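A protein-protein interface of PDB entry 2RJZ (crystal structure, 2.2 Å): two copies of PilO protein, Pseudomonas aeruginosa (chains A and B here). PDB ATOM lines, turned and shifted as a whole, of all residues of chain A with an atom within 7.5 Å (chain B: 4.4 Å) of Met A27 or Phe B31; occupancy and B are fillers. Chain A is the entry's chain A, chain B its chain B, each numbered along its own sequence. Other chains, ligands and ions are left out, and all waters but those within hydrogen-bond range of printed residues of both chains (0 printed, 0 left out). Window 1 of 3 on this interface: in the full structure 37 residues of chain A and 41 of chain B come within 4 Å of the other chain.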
ATOM      1  N   LEU A   3       7.552  14.775  -3.073  1.00  0.00           N
ATOM      2  CA  LEU A   3       8.872  14.689  -3.698  1.00  0.00           C
ATOM      3  C   LEU A   3       8.917  15.417  -5.061  1.00  0.00           C
ATOM      4  O   LEU A   3       9.884  16.125  -5.353  1.00  0.00           O
ATOM      5  CB  LEU A   3       9.271  13.221  -3.866  1.00  0.00           C
ATOM      6  CG  LEU A   3      10.705  12.856  -4.263  1.00  0.00           C
ATOM      7  CD1 LEU A   3      11.709  13.542  -3.329  1.00  0.00           C
ATOM      8  CD2 LEU A   3      10.876  11.307  -4.277  1.00  0.00           C
ATOM      9  N   LYS A   4       7.870  15.238  -5.876  1.00  0.00           N
ATOM     10  CA  LYS A   4       7.757  15.883  -7.179  1.00  0.00           C
ATOM     11  C   LYS A   4       7.675  17.406  -7.064  1.00  0.00           C
ATOM     12  O   LYS A   4       8.249  18.135  -7.884  1.00  0.00           O
ATOM     13  CB  LYS A   4       6.512  15.378  -7.930  1.00  0.00           C
ATOM     14  CG  LYS A   4       6.312  16.080  -9.268  1.00  0.00           C
ATOM     15  CD  LYS A   4       5.138  15.523 -10.045  1.00  0.00           C
ATOM     16  CE  LYS A   4       4.910  16.343 -11.289  1.00  0.00           C
ATOM     17  NZ  LYS A   4       4.001  15.647 -12.256  1.00  0.00           N
ATOM     18  N   PHE A   7      11.320  18.452  -6.447  1.00  0.00           N
ATOM     19  CA  PHE A   7      12.089  18.559  -7.702  1.00  0.00           C
ATOM     20  C   PHE A   7      11.620  19.696  -8.598  1.00  0.00           C
ATOM     21  O   PHE A   7      12.469  20.363  -9.182  1.00  0.00           O
ATOM     22  CB  PHE A   7      12.147  17.240  -8.488  1.00  0.00           C
ATOM     23  CG  PHE A   7      13.053  16.224  -7.871  1.00  0.00           C
ATOM     24  CD1 PHE A   7      14.438  16.447  -7.820  1.00  0.00           C
ATOM     25  CD2 PHE A   7      12.530  15.069  -7.300  1.00  0.00           C
ATOM     26  CE1 PHE A   7      15.286  15.528  -7.237  1.00  0.00           C
ATOM     27  CE2 PHE A   7      13.384  14.128  -6.713  1.00  0.00           C
ATOM     28  CZ  PHE A   7      14.767  14.359  -6.680  1.00  0.00           C
ATOM     29  N   LYS A  21      13.848  17.996 -16.582  1.00  0.00           N
ATOM     30  CA  LYS A  21      12.437  17.693 -16.807  1.00  0.00           C
ATOM     31  C   LYS A  21      12.246  16.311 -17.381  1.00  0.00           C
ATOM     32  O   LYS A  21      11.282  15.634 -17.029  1.00  0.00           O
ATOM     33  CB  LYS A  21      11.797  18.690 -17.763  1.00  0.00           C
ATOM     34  CG  LYS A  21      11.459  20.035 -17.175  1.00  0.00           C
ATOM     35  CD  LYS A  21      11.279  21.013 -18.331  1.00  0.00           C
ATOM     36  CE  LYS A  21       9.971  21.761 -18.246  1.00  0.00           C
ATOM     37  NZ  LYS A  21      10.059  23.015 -19.044  1.00  0.00           N
ATOM     38  N   ALA A  22      13.147  15.904 -18.284  1.00  0.00           N
ATOM     39  CA  ALA A  22      13.043  14.621 -18.979  1.00  0.00           C
ATOM     40  C   ALA A  22      13.261  13.505 -17.985  1.00  0.00           C
ATOM     41  O   ALA A  22      12.600  12.480 -18.056  1.00  0.00           O
ATOM     42  CB  ALA A  22      14.078  14.523 -20.154  1.00  0.00           C
ATOM     43  N   GLN A  23      14.184  13.705 -17.047  1.00  0.00           N
ATOM     44  CA  GLN A  23      14.370  12.728 -15.946  1.00  0.00           C
ATOM     45  C   GLN A  23      13.225  12.698 -14.915  1.00  0.00           C
ATOM     46  O   GLN A  23      12.854  11.636 -14.412  1.00  0.00           O
ATOM     47  CB  GLN A  23      15.725  12.959 -15.263  1.00  0.00           C
ATOM     48  CG  GLN A  23      16.922  12.646 -16.178  1.00  0.00           C
ATOM     49  CD  GLN A  23      17.179  11.135 -16.442  1.00  0.00           C
ATOM     50  OE1 GLN A  23      16.479  10.239 -15.936  1.00  0.00           O
ATOM     51  NE2 GLN A  23      18.215  10.861 -17.244  1.00  0.00           N
ATOM     52  N   MET A  24      12.657  13.865 -14.599  1.00  0.00           N
ATOM     53  CA  MET A  24      11.469  13.910 -13.718  1.00  0.00           C
ATOM     54  C   MET A  24      10.407  13.027 -14.383  1.00  0.00           C
ATOM     55  O   MET A  24       9.789  12.179 -13.736  1.00  0.00           O
ATOM     56  CB  MET A  24      10.931  15.343 -13.540  1.00  0.00           C
ATOM     57  CG  MET A  24      11.698  16.266 -12.546  1.00  0.00           C
ATOM     58  SD  MET A  24      10.898  17.890 -12.397  1.00  0.00           S
ATOM     59  CE  MET A  24       9.483  17.353 -11.422  1.00  0.00           C
ATOM     60  N   LYS A  25      10.216  13.231 -15.682  1.00  0.00           N
ATOM     61  CA  LYS A  25       9.190  12.505 -16.441  1.00  0.00           C
ATOM     62  C   LYS A  25       9.461  10.972 -16.516  1.00  0.00           C
ATOM     63  O   LYS A  25       8.509  10.180 -16.446  1.00  0.00           O
ATOM     64  CB  LYS A  25       9.023  13.143 -17.821  1.00  0.00           C
ATOM     65  CG  LYS A  25       8.105  12.420 -18.765  1.00  0.00           C
ATOM     66  CD  LYS A  25       8.184  13.017 -20.177  1.00  0.00           C
ATOM     67  CE  LYS A  25       7.069  12.454 -21.086  1.00  0.00           C
ATOM     68  NZ  LYS A  25       7.382  12.716 -22.522  1.00  0.00           N
ATOM     69  N   GLU A  26      10.727  10.564 -16.612  1.00  0.00           N
ATOM     70  CA  GLU A  26      11.097   9.132 -16.579  1.00  0.00           C
ATOM     71  C   GLU A  26      10.962   8.442 -15.189  1.00  0.00           C
ATOM     72  O   GLU A  26      10.575   7.270 -15.089  1.00  0.00           O
ATOM     73  CB  GLU A  26      12.501   8.946 -17.138  1.00  0.00           C
ATOM     74  CG  GLU A  26      12.515   8.862 -18.696  1.00  0.00           C
ATOM     75  CD  GLU A  26      13.845   9.297 -19.327  1.00  0.00           C
ATOM     76  OE1 GLU A  26      14.922   9.031 -18.724  1.00  0.00           O
ATOM     77  OE2 GLU A  26      13.808   9.906 -20.436  1.00  0.00           O
ATOM     78  N   MET A  27      11.282   9.181 -14.124  1.00  0.00           N
ATOM     79  CA  MET A  27      10.999   8.741 -12.759  1.00  0.00           C
ATOM     80  C   MET A  27       9.491   8.509 -12.595  1.00  0.00           C
ATOM     81  O   MET A  27       9.059   7.454 -12.110  1.00  0.00           O
ATOM     82  CB  MET A  27      11.515   9.773 -11.748  1.00  0.00           C
ATOM     83  CG  MET A  27      11.743   9.218 -10.371  1.00  0.00           C
ATOM     84  SD  MET A  27      12.434  10.371  -9.165  1.00  0.00           S
ATOM     85  CE  MET A  27      12.179   9.302  -7.766  1.00  0.00           C
ATOM     86  N   GLU A  28       8.701   9.499 -12.999  1.00  0.00           N
ATOM     87  CA  GLU A  28       7.241   9.403 -12.916  1.00  0.00           C
ATOM     88  C   GLU A  28       6.695   8.244 -13.743  1.00  0.00           C
ATOM     89  O   GLU A  28       5.860   7.478 -13.267  1.00  0.00           O
ATOM     90  CB  GLU A  28       6.593  10.709 -13.361  1.00  0.00           C
ATOM     91  CG  GLU A  28       7.073  11.881 -12.552  1.00  0.00           C
ATOM     92  CD  GLU A  28       6.374  13.158 -12.930  1.00  0.00           C
ATOM     93  OE1 GLU A  28       5.113  13.175 -12.830  1.00  0.00           O
ATOM     94  OE2 GLU A  28       7.094  14.123 -13.314  1.00  0.00           O
ATOM     95  N   GLU A  29       7.175   8.117 -14.977  1.00  0.00           N
ATOM     96  CA  GLU A  29       6.711   7.064 -15.870  1.00  0.00           C
ATOM     97  C   GLU A  29       7.021   5.680 -15.274  1.00  0.00           C
ATOM     98  O   GLU A  29       6.167   4.780 -15.272  1.00  0.00           O
ATOM     99  CB  GLU A  29       7.325   7.236 -17.274  1.00  0.00           C
ATOM    100  CG  GLU A  29       6.706   6.321 -18.336  1.00  0.00           C
ATOM    101  CD  GLU A  29       6.918   6.842 -19.765  1.00  0.00           C
ATOM    102  OE1 GLU A  29       7.901   7.609 -19.996  1.00  0.00           O
ATOM    103  OE2 GLU A  29       6.098   6.482 -20.646  1.00  0.00           O
ATOM    104  N   SER A  30       8.239   5.529 -14.758  1.00  0.00           N
ATOM    105  CA  SER A  30       8.636   4.321 -14.057  1.00  0.00           C
ATOM    106  C   SER A  30       7.788   4.034 -12.827  1.00  0.00           C
ATOM    107  O   SER A  30       7.425   2.891 -12.583  1.00  0.00           O
ATOM    108  CB  SER A  30      10.113   4.385 -13.687  1.00  0.00           C
ATOM    109  OG  SER A  30      10.873   4.356 -14.886  1.00  0.00           O
ATOM    110  N   PHE A  31       7.451   5.065 -12.068  1.00  0.00           N
ATOM    111  CA  PHE A  31       6.608   4.881 -10.899  1.00  0.00           C
ATOM    112  C   PHE A  31       5.236   4.344 -11.342  1.00  0.00           C
ATOM    113  O   PHE A  31       4.739   3.399 -10.767  1.00  0.00           O
ATOM    114  CB  PHE A  31       6.500   6.196 -10.115  1.00  0.00           C
ATOM    115  CG  PHE A  31       5.673   6.105  -8.838  1.00  0.00           C
ATOM    116  CD1 PHE A  31       5.922   5.115  -7.873  1.00  0.00           C
ATOM    117  CD2 PHE A  31       4.678   7.038  -8.593  1.00  0.00           C
ATOM    118  CE1 PHE A  31       5.187   5.075  -6.665  1.00  0.00           C
ATOM    119  CE2 PHE A  31       3.920   6.997  -7.420  1.00  0.00           C
ATOM    120  CZ  PHE A  31       4.172   6.007  -6.454  1.00  0.00           C
ATOM    121  N   GLY A  32       4.650   4.944 -12.379  1.00  0.00           N
ATOM    122  CA  GLY A  32       3.394   4.478 -12.957  1.00  0.00           C
ATOM    123  C   GLY A  32       3.488   3.071 -13.541  1.00  0.00           C
ATOM    124  O   GLY A  32       2.582   2.292 -13.366  1.00  0.00           O
ATOM    125  N   ALA A  33       4.573   2.741 -14.236  1.00  0.00           N
ATOM    126  CA  ALA A  33       4.736   1.378 -14.768  1.00  0.00           C
ATOM    127  C   ALA A  33       4.757   0.349 -13.633  1.00  0.00           C
ATOM    128  O   ALA A  33       4.136  -0.718 -13.756  1.00  0.00           O
ATOM    129  CB  ALA A  33       5.983   1.266 -15.625  1.00  0.00           C
ATOM    130  N   LEU A  34       5.416   0.679 -12.514  1.00  0.00           N
ATOM    131  CA  LEU A  34       5.369  -0.213 -11.328  1.00  0.00           C
ATOM    132  C   LEU A  34       3.967  -0.389 -10.759  1.00  0.00           C
ATOM    133  O   LEU A  34       3.563  -1.503 -10.453  1.00  0.00           O
ATOM    134  CB  LEU A  34       6.296   0.269 -10.213  1.00  0.00           C
ATOM    135  CG  LEU A  34       7.792   0.128 -10.399  1.00  0.00           C
ATOM    136  CD1 LEU A  34       8.527   1.041  -9.404  1.00  0.00           C
ATOM    137  CD2 LEU A  34       8.184  -1.359 -10.244  1.00  0.00           C
ATOM    138  N   PHE A  75       1.286  10.140 -14.994  1.00  0.00           N
ATOM    139  CA  PHE A  75       1.356   8.676 -15.041  1.00  0.00           C
ATOM    140  C   PHE A  75       0.819   7.948 -13.806  1.00  0.00           C
ATOM    141  O   PHE A  75       0.815   6.716 -13.753  1.00  0.00           O
ATOM    142  CB  PHE A  75       2.780   8.213 -15.398  1.00  0.00           C
ATOM    143  CG  PHE A  75       3.288   8.781 -16.706  1.00  0.00           C
ATOM    144  CD1 PHE A  75       2.839   8.283 -17.915  1.00  0.00           C
ATOM    145  CD2 PHE A  75       4.206   9.810 -16.716  1.00  0.00           C
ATOM    146  CE1 PHE A  75       3.291   8.813 -19.127  1.00  0.00           C
ATOM    147  CE2 PHE A  75       4.670  10.331 -17.894  1.00  0.00           C
ATOM    148  CZ  PHE A  75       4.216   9.845 -19.106  1.00  0.00           C
ATOM    149  N   TYR A  76       0.382   8.709 -12.813  1.00  0.00           N
ATOM    150  CA  TYR A  76      -0.134   8.138 -11.579  1.00  0.00           C
ATOM    151  C   TYR A  76      -1.085   9.132 -10.954  1.00  0.00           C
ATOM    152  O   TYR A  76      -1.032  10.334 -11.229  1.00  0.00           O
ATOM    153  CB  TYR A  76       1.000   7.760 -10.600  1.00  0.00           C
ATOM    154  CG  TYR A  76       1.734   8.957 -10.021  1.00  0.00           C
ATOM    155  CD1 TYR A  76       1.314   9.557  -8.850  1.00  0.00           C
ATOM    156  CD2 TYR A  76       2.856   9.486 -10.669  1.00  0.00           C
ATOM    157  CE1 TYR A  76       1.990  10.671  -8.330  1.00  0.00           C
ATOM    158  CE2 TYR A  76       3.519  10.584 -10.169  1.00  0.00           C
ATOM    159  CZ  TYR A  76       3.087  11.171  -9.010  1.00  0.00           C
ATOM    160  OH  TYR A  76       3.764  12.256  -8.524  1.00  0.00           O
ATOM    161  N   MET B  27      13.621   3.629 -11.936  1.00  0.00           N
ATOM    162  CA  MET B  27      13.112   4.624 -11.009  1.00  0.00           C
ATOM    163  C   MET B  27      14.257   5.211 -10.182  1.00  0.00           C
ATOM    164  O   MET B  27      14.406   6.438 -10.104  1.00  0.00           O
ATOM    165  CB  MET B  27      12.022   4.039 -10.122  1.00  0.00           C
ATOM    166  CG  MET B  27      11.022   5.099  -9.664  1.00  0.00           C
ATOM    167  SD  MET B  27       9.735   4.506  -8.550  1.00  0.00           S
ATOM    168  CE  MET B  27       9.381   6.134  -7.857  1.00  0.00           C
ATOM    169  N   GLU B  28      15.074   4.342  -9.599  1.00  0.00           N
ATOM    170  CA  GLU B  28      16.250   4.763  -8.814  1.00  0.00           C
ATOM    171  C   GLU B  28      17.287   5.524  -9.608  1.00  0.00           C
ATOM    172  O   GLU B  28      17.888   6.467  -9.093  1.00  0.00           O
ATOM    173  CB  GLU B  28      16.947   3.557  -8.218  1.00  0.00           C
ATOM    174  CG  GLU B  28      16.176   2.929  -7.105  1.00  0.00           C
ATOM    175  CD  GLU B  28      16.855   1.689  -6.579  1.00  0.00           C
ATOM    176  OE1 GLU B  28      17.797   1.812  -5.770  1.00  0.00           O
ATOM    177  OE2 GLU B  28      16.429   0.590  -6.983  1.00  0.00           O
ATOM    178  N   GLU B  29      17.518   5.072 -10.849  1.00  0.00           N
ATOM    179  CA  GLU B  29      18.470   5.692 -11.764  1.00  0.00           C
ATOM    180  C   GLU B  29      18.079   7.114 -12.090  1.00  0.00           C
ATOM    181  O   GLU B  29      18.941   7.982 -12.134  1.00  0.00           O
ATOM    182  CB  GLU B  29      18.535   4.939 -13.079  1.00  0.00           C
ATOM    183  CG  GLU B  29      19.599   3.888 -13.126  1.00  0.00           C
ATOM    184  CD  GLU B  29      20.040   3.528 -14.540  1.00  0.00           C
ATOM    185  OE1 GLU B  29      20.460   4.445 -15.290  1.00  0.00           O
ATOM    186  OE2 GLU B  29      19.978   2.318 -14.884  1.00  0.00           O
ATOM    187  N   SER B  30      16.793   7.321 -12.379  1.00  0.00           N
ATOM    188  CA  SER B  30      16.254   8.647 -12.646  1.00  0.00           C
ATOM    189  C   SER B  30      16.368   9.535 -11.418  1.00  0.00           C
ATOM    190  O   SER B  30      16.784  10.687 -11.524  1.00  0.00           O
ATOM    191  CB  SER B  30      14.806   8.533 -13.095  1.00  0.00           C
ATOM    192  OG  SER B  30      14.750   7.768 -14.292  1.00  0.00           O
ATOM    193  N   PHE B  31      16.043   8.981 -10.249  1.00  0.00           N
ATOM    194  CA  PHE B  31      16.237   9.696  -9.000  1.00  0.00           C
ATOM    195  C   PHE B  31      17.712  10.136  -8.885  1.00  0.00           C
ATOM    196  O   PHE B  31      18.006  11.323  -8.668  1.00  0.00           O
ATOM    197  CB  PHE B  31      15.800   8.811  -7.844  1.00  0.00           C
ATOM    198  CG  PHE B  31      15.846   9.464  -6.503  1.00  0.00           C
ATOM    199  CD1 PHE B  31      15.145  10.634  -6.248  1.00  0.00           C
ATOM    200  CD2 PHE B  31      16.539   8.855  -5.456  1.00  0.00           C
ATOM    201  CE1 PHE B  31      15.146  11.205  -4.994  1.00  0.00           C
ATOM    202  CE2 PHE B  31      16.547   9.431  -4.196  1.00  0.00           C
ATOM    203  CZ  PHE B  31      15.841  10.600  -3.967  1.00  0.00           C
ATOM    204  N   GLY B  32      18.623   9.185  -9.106  1.00  0.00           N
ATOM    205  CA  GLY B  32      20.072   9.448  -9.096  1.00  0.00           C
ATOM    206  C   GLY B  32      20.488  10.539 -10.073  1.00  0.00           C
ATOM    207  O   GLY B  32      21.308  11.398  -9.728  1.00  0.00           O
ATOM    208  N   ALA B  33      19.915  10.517 -11.280  1.00  0.00           N
ATOM    209  CA  ALA B  33      20.205  11.535 -12.308  1.00  0.00           C
ATOM    210  C   ALA B  33      19.690  12.950 -11.978  1.00  0.00           C
ATOM    211  O   ALA B  33      20.336  13.945 -12.323  1.00  0.00           O
ATOM    212  CB  ALA B  33      19.697  11.095 -13.633  1.00  0.00           C
ATOM    213  N   LEU B  34      18.553  13.054 -11.287  1.00  0.00           N
ATOM    214  CA  LEU B  34      18.048  14.378 -10.875  1.00  0.00           C
ATOM    215  C   LEU B  34      18.904  14.989  -9.766  1.00  0.00           C
ATOM    216  O   LEU B  34      19.203  16.173  -9.807  1.00  0.00           O
ATOM    217  CB  LEU B  34      16.585  14.313 -10.426  1.00  0.00           C
ATOM    218  CG  LEU B  34      15.505  13.874 -11.414  1.00  0.00           C
ATOM    219  CD1 LEU B  34      14.306  13.286 -10.644  1.00  0.00           C
ATOM    220  CD2 LEU B  34      15.085  15.037 -12.334  1.00  0.00           C
ATOM    221  N   LEU B  35      19.298  14.187  -8.783  1.00  0.00           N
ATOM    222  CA  LEU B  35      20.240  14.647  -7.755  1.00  0.00           C
ATOM    223  C   LEU B  35      21.588  15.163  -8.306  1.00  0.00           C
ATOM    224  O   LEU B  35      22.167  16.094  -7.752  1.00  0.00           O
ATOM    225  CB  LEU B  35      20.495  13.538  -6.732  1.00  0.00           C
ATOM    226  CG  LEU B  35      19.243  13.050  -6.001  1.00  0.00           C
ATOM    227  CD1 LEU B  35      19.566  11.738  -5.265  1.00  0.00           C
ATOM    228  CD2 LEU B  35      18.678  14.138  -5.083  1.00  0.00           C
ATOM    229  N   TYR B  76      22.054   6.389  -5.610  1.00  0.00           N
ATOM    230  CA  TYR B  76      21.957   7.544  -4.709  1.00  0.00           C
ATOM    231  C   TYR B  76      22.419   7.161  -3.311  1.00  0.00           C
ATOM    232  O   TYR B  76      22.419   5.979  -2.955  1.00  0.00           O
ATOM    233  CB  TYR B  76      20.513   8.096  -4.641  1.00  0.00           C
ATOM    234  CG  TYR B  76      19.473   7.070  -4.196  1.00  0.00           C
ATOM    235  CD1 TYR B  76      19.148   6.898  -2.841  1.00  0.00           C
ATOM    236  CD2 TYR B  76      18.833   6.255  -5.135  1.00  0.00           C
ATOM    237  CE1 TYR B  76      18.202   5.953  -2.452  1.00  0.00           C
ATOM    238  CE2 TYR B  76      17.887   5.340  -4.766  1.00  0.00           C
ATOM    239  CZ  TYR B  76      17.574   5.176  -3.443  1.00  0.00           C
ATOM    240  OH  TYR B  76      16.647   4.207  -3.118  1.00  0.00           O
ATOM    241  N   TYR B 133      19.545  13.301   0.293  1.00  0.00           N
ATOM    242  CA  TYR B 133      20.085  12.339  -0.653  1.00  0.00           C
ATOM    243  C   TYR B 133      21.082  12.988  -1.585  1.00  0.00           C
ATOM    244  O   TYR B 133      20.981  14.156  -1.875  1.00  0.00           O
ATOM    245  CB  TYR B 133      18.969  11.711  -1.508  1.00  0.00           C
ATOM    246  CG  TYR B 133      17.829  11.135  -0.710  1.00  0.00           C
ATOM    247  CD1 TYR B 133      17.739   9.766  -0.465  1.00  0.00           C
ATOM    248  CD2 TYR B 133      16.844  11.972  -0.187  1.00  0.00           C
ATOM    249  CE1 TYR B 133      16.676   9.231   0.290  1.00  0.00           C
ATOM    250  CE2 TYR B 133      15.782  11.467   0.579  1.00  0.00           C
ATOM    251  CZ  TYR B 133      15.704  10.101   0.812  1.00  0.00           C
ATOM    252  OH  TYR B 133      14.641   9.648   1.542  1.00  0.00           O
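Hydrophobic or aromatic side chains of chain A that line the printed part of chain B: Phe A7, Met A24, Met A27, Phe A31 and Leu A34. Among the printed residues, 14 pairs touch across the chains. Among the printed residues, no Asp or Glu carboxylate lies within 4 Å of a Lys or Arg side-chain nitrogen of the other chain.
The side-chain hydroxyl (OG) of Ser B30 is in hydrogen-bond range of the side-chain amide oxygen (OE1) of Gln A23 (3.4 Å).
The side-chain amide oxygen (OE1) of Gln A23 sits close to the side-chain carboxylate (OE1) of Glu A26, at 3.4 Å. The backbone carbonyl oxygen of Glu A26 lies within hydrogen-bond range of the side-chain hydroxyl of Ser A30, at 2.9 Å.
Met A27 touches its own counterpart, Met B27. Met A27 touches Ser B30, and with the chains exchanged Ser A30 touches Met B27. Met A27 touches Phe B31, and with the chains exchanged Phe A31 touches Met B27. Met A27 touches Leu B34, and with the chains exchanged Leu A34 touches Met B27. Of the 14 pairs that touch across the chains among the printed residues, 7 have their exchanged pair printed and touching as well.
Phe B31 touches Phe A7 (CE1 to CZ, 3.6 Å). Ala B33 touches Gln A23 (CB to CD, 3.8 Å). N of Met A24 touches CD2 of Leu B34 (3.5 Å). Ser B30 touches Glu A26. Ser B30 touches Met A27 (CB to N, 3.7 Å). Phe B31 touches Met A27. Leu B34 touches Met A27. N of Met B27 touches CB of Ser A30, 3.99 Å away. Phe A31 touches Met B27 (CD1 to CE, 3.6 Å). Leu A34 touches Met B27 (CD1 to SD, 3.8 Å).
Met A27 touches just these residues of chain B: Met B27, Ser B30, Phe B31 and Leu B34. Of chain A, only Phe A7 and Met A27 come within 4 Å of Phe B31. Printed residues of chain B within 4 Å of Met A24: Leu B34 (3.5 Å). Of the printed residues of chain B, Phe A7 touches Phe B31 (3.6 Å) and Leu B34 (3.7 Å). Of the printed residues of chain A, Met B27 touches Met A27 (3.9 Å), Ser A30 (3.99 Å), Phe A31 (3.6 Å) and Leu A34 (3.8 Å). Leu B35 touches none of the printed residues of chain A. The nearest residue of chain A that does not touch Phe B31 is Leu A3 (4.3 Å). The nearest printed residue of chain A that does not touch Met B27 is Glu A26 (5.5 Å).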
